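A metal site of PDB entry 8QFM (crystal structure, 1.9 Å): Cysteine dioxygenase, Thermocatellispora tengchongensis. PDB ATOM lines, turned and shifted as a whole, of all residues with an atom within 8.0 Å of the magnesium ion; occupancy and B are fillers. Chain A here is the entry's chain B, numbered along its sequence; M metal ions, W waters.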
ATOM      1  N   GLY A  21      19.114 -24.690  37.146  1.00  0.00           N
ATOM      2  CA  GLY A  21      20.564 -24.571  36.796  1.00  0.00           C
ATOM      3  C   GLY A  21      20.784 -24.534  35.294  1.00  0.00           C
ATOM      4  O   GLY A  21      20.068 -25.189  34.543  1.00  0.00           O
ATOM      5  N   GLU A  22      21.774 -23.754  34.858  1.00  0.00           N
ATOM      6  CA  GLU A  22      22.115 -23.685  33.446  1.00  0.00           C
ATOM      7  C   GLU A  22      22.433 -25.066  32.913  1.00  0.00           C
ATOM      8  O   GLU A  22      23.054 -25.896  33.600  1.00  0.00           O
ATOM      9  CB  GLU A  22      23.292 -22.744  33.213  1.00  0.00           C
ATOM     10  CG  GLU A  22      23.506 -22.321  31.775  1.00  0.00           C
ATOM     11  CD  GLU A  22      22.203 -21.924  31.073  1.00  0.00           C
ATOM     12  OE1 GLU A  22      21.637 -20.854  31.348  1.00  0.00           O
ATOM     13  OE2 GLU A  22      21.702 -22.693  30.239  1.00  0.00           O
ATOM     14  N   LEU A  23      22.020 -25.323  31.666  1.00  0.00           N
ATOM     15  CA  LEU A  23      22.303 -26.582  30.991  1.00  0.00           C
ATOM     16  C   LEU A  23      23.167 -26.329  29.767  1.00  0.00           C
ATOM     17  O   LEU A  23      22.858 -25.465  28.949  1.00  0.00           O
ATOM     18  CB  LEU A  23      21.000 -27.276  30.582  1.00  0.00           C
ATOM     19  CG  LEU A  23      20.035 -27.603  31.723  1.00  0.00           C
ATOM     20  CD1 LEU A  23      18.702 -28.112  31.211  1.00  0.00           C
ATOM     21  CD2 LEU A  23      20.700 -28.638  32.630  1.00  0.00           C
ATOM     22  N   ASP A  24      24.259 -27.081  29.670  1.00  0.00           N
ATOM     23  CA  ASP A  24      25.144 -27.071  28.502  1.00  0.00           C
ATOM     24  C   ASP A  24      24.437 -27.761  27.347  1.00  0.00           C
ATOM     25  O   ASP A  24      24.460 -28.989  27.228  1.00  0.00           O
ATOM     26  CB  ASP A  24      26.459 -27.771  28.876  1.00  0.00           C
ATOM     27  CG  ASP A  24      27.500 -27.670  27.785  1.00  0.00           C
ATOM     28  OD1 ASP A  24      27.163 -27.285  26.648  1.00  0.00           O
ATOM     29  OD2 ASP A  24      28.674 -27.994  28.078  1.00  0.00           O
ATOM     30  N   LEU A  25      23.775 -26.968  26.506  1.00  0.00           N
ATOM     31  CA  LEU A  25      22.954 -27.479  25.415  1.00  0.00           C
ATOM     32  C   LEU A  25      23.193 -26.635  24.174  1.00  0.00           C
ATOM     33  O   LEU A  25      23.543 -25.450  24.277  1.00  0.00           O
ATOM     34  CB  LEU A  25      21.456 -27.428  25.760  1.00  0.00           C
ATOM     35  CG  LEU A  25      20.979 -28.404  26.823  1.00  0.00           C
ATOM     36  CD1 LEU A  25      19.574 -27.988  27.271  1.00  0.00           C
ATOM     37  CD2 LEU A  25      20.989 -29.824  26.297  1.00  0.00           C
ATOM     38  N   PRO A  26      23.007 -27.210  22.984  1.00  0.00           N
ATOM     39  CA  PRO A  26      23.016 -26.391  21.767  1.00  0.00           C
ATOM     40  C   PRO A  26      22.094 -25.195  21.921  1.00  0.00           C
ATOM     41  O   PRO A  26      21.034 -25.268  22.541  1.00  0.00           O
ATOM     42  CB  PRO A  26      22.503 -27.336  20.677  1.00  0.00           C
ATOM     43  CG  PRO A  26      22.702 -28.706  21.202  1.00  0.00           C
ATOM     44  CD  PRO A  26      22.780 -28.649  22.704  1.00  0.00           C
ATOM     45  N   GLU A  27      22.502 -24.067  21.334  1.00  0.00           N
ATOM     46  CA  GLU A  27      21.742 -22.823  21.458  1.00  0.00           C
ATOM     47  C   GLU A  27      20.684 -22.754  20.355  1.00  0.00           C
ATOM     48  O   GLU A  27      20.738 -21.953  19.421  1.00  0.00           O
ATOM     49  CB  GLU A  27      22.683 -21.634  21.428  1.00  0.00           C
ATOM     50  CG  GLU A  27      23.581 -21.583  22.651  1.00  0.00           C
ATOM     51  CD  GLU A  27      24.825 -22.442  22.503  1.00  0.00           C
ATOM     52  OE1 GLU A  27      25.555 -22.596  23.504  1.00  0.00           O
ATOM     53  OE2 GLU A  27      25.106 -22.948  21.402  1.00  0.00           O
ATOM     54  N   HIS A  67      15.131 -26.024  34.457  1.00  0.00           N
ATOM     55  CA  HIS A  67      15.729 -24.973  33.624  1.00  0.00           C
ATOM     56  C   HIS A  67      14.651 -24.574  32.637  1.00  0.00           C
ATOM     57  O   HIS A  67      13.919 -25.419  32.117  1.00  0.00           O
ATOM     58  CB  HIS A  67      17.023 -25.439  32.893  1.00  0.00           C
ATOM     59  CG  HIS A  67      17.784 -24.340  32.162  1.00  0.00           C
ATOM     60  ND1 HIS A  67      18.301 -23.224  32.790  1.00  0.00           N
ATOM     61  CD2 HIS A  67      18.179 -24.248  30.867  1.00  0.00           C
ATOM     62  CE1 HIS A  67      18.935 -22.474  31.907  1.00  0.00           C
ATOM     63  NE2 HIS A  67      18.875 -23.067  30.721  1.00  0.00           N
ATOM     64  N   ARG A  68      14.500 -23.268  32.432  1.00  0.00           N
ATOM     65  CA  ARG A  68      13.671 -22.721  31.362  1.00  0.00           C
ATOM     66  C   ARG A  68      14.489 -21.606  30.732  1.00  0.00           C
ATOM     67  O   ARG A  68      15.085 -20.797  31.455  1.00  0.00           O
ATOM     68  CB  ARG A  68      12.324 -22.212  31.874  1.00  0.00           C
ATOM     69  CG  ARG A  68      11.747 -23.088  32.959  1.00  0.00           C
ATOM     70  CD  ARG A  68      10.380 -22.636  33.429  1.00  0.00           C
ATOM     71  NE  ARG A  68       9.461 -22.322  32.352  1.00  0.00           N
ATOM     72  CZ  ARG A  68       8.236 -21.834  32.544  1.00  0.00           C
ATOM     73  NH1 ARG A  68       7.801 -21.605  33.769  1.00  0.00           N
ATOM     74  NH2 ARG A  68       7.456 -21.576  31.508  1.00  0.00           N
ATOM     75  N   ASP A  69      14.571 -21.607  29.408  1.00  0.00           N
ATOM     76  CA  ASP A  69      15.263 -20.540  28.707  1.00  0.00           C
ATOM     77  C   ASP A  69      14.545 -20.359  27.377  1.00  0.00           C
ATOM     78  O   ASP A  69      13.380 -20.733  27.233  1.00  0.00           O
ATOM     79  CB  ASP A  69      16.776 -20.838  28.600  1.00  0.00           C
ATOM     80  CG  ASP A  69      17.105 -22.091  27.798  1.00  0.00           C
ATOM     81  OD1 ASP A  69      16.276 -22.601  27.013  1.00  0.00           O
ATOM     82  OD2 ASP A  69      18.267 -22.563  27.955  1.00  0.00           O
ATOM     83  N   ALA A  70      15.214 -19.744  26.402  1.00  0.00           N
ATOM     84  CA  ALA A  70      14.560 -19.481  25.129  1.00  0.00           C
ATOM     85  C   ALA A  70      14.275 -20.752  24.355  1.00  0.00           C
ATOM     86  O   ALA A  70      13.452 -20.736  23.429  1.00  0.00           O
ATOM     87  CB  ALA A  70      15.411 -18.536  24.283  1.00  0.00           C
ATOM     88  N   TYR A  71      14.913 -21.853  24.715  1.00  0.00           N
ATOM     89  CA  TYR A  71      14.900 -23.064  23.902  1.00  0.00           C
ATOM     90  C   TYR A  71      14.228 -24.245  24.565  1.00  0.00           C
ATOM     91  O   TYR A  71      13.561 -25.031  23.873  1.00  0.00           O
ATOM     92  CB  TYR A  71      16.350 -23.437  23.549  1.00  0.00           C
ATOM     93  CG  TYR A  71      17.086 -22.310  22.891  1.00  0.00           C
ATOM     94  CD1 TYR A  71      16.672 -21.836  21.652  1.00  0.00           C
ATOM     95  CD2 TYR A  71      18.183 -21.714  23.495  1.00  0.00           C
ATOM     96  CE1 TYR A  71      17.339 -20.789  21.036  1.00  0.00           C
ATOM     97  CE2 TYR A  71      18.850 -20.668  22.879  1.00  0.00           C
ATOM     98  CZ  TYR A  71      18.420 -20.204  21.655  1.00  0.00           C
ATOM     99  OH  TYR A  71      19.091 -19.161  21.047  1.00  0.00           O
ATOM    100  N   VAL A  72      14.368 -24.406  25.875  1.00  0.00           N
ATOM    101  CA  VAL A  72      13.863 -25.583  26.570  1.00  0.00           C
ATOM    102  C   VAL A  72      13.150 -25.178  27.851  1.00  0.00           C
ATOM    103  O   VAL A  72      13.410 -24.124  28.439  1.00  0.00           O
ATOM    104  CB  VAL A  72      15.008 -26.586  26.893  1.00  0.00           C
ATOM    105  CG1 VAL A  72      15.758 -26.978  25.637  1.00  0.00           C
ATOM    106  CG2 VAL A  72      15.959 -26.000  27.933  1.00  0.00           C
HETATM  107 MG    MG M   1      19.903 -22.317  29.294  1.00  0.00          MG
HETATM  108  O   HOH W   1      20.424 -24.239  28.484  1.00  0.00           O
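OD1 of Asp 69 lies within hydrogen-bond range of N of Val 72, 2.9 Å away.
ND1 of His 67 is in hydrogen-bond range of O of Gly 21 (3.2 Å).
N of Tyr 71 sits at hydrogen-bond distance from OD1 of Asp 69, at 2.8 Å.
Within 4 Å of the magnesium ion: Glu 22, His 67 and Asp 69.
The nearest printed residue that does not touch the magnesium ion is Leu 23 (4.3 Å).
The magnesium ion is bound by NE2 of His 67 (1.9 Å), OE2 of Glu 22 (2.1 Å), OD2 of Asp 69 (2.1 Å) and water W1 (2.1 Å).
The magnesium ion has four donor atoms within binding distance.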
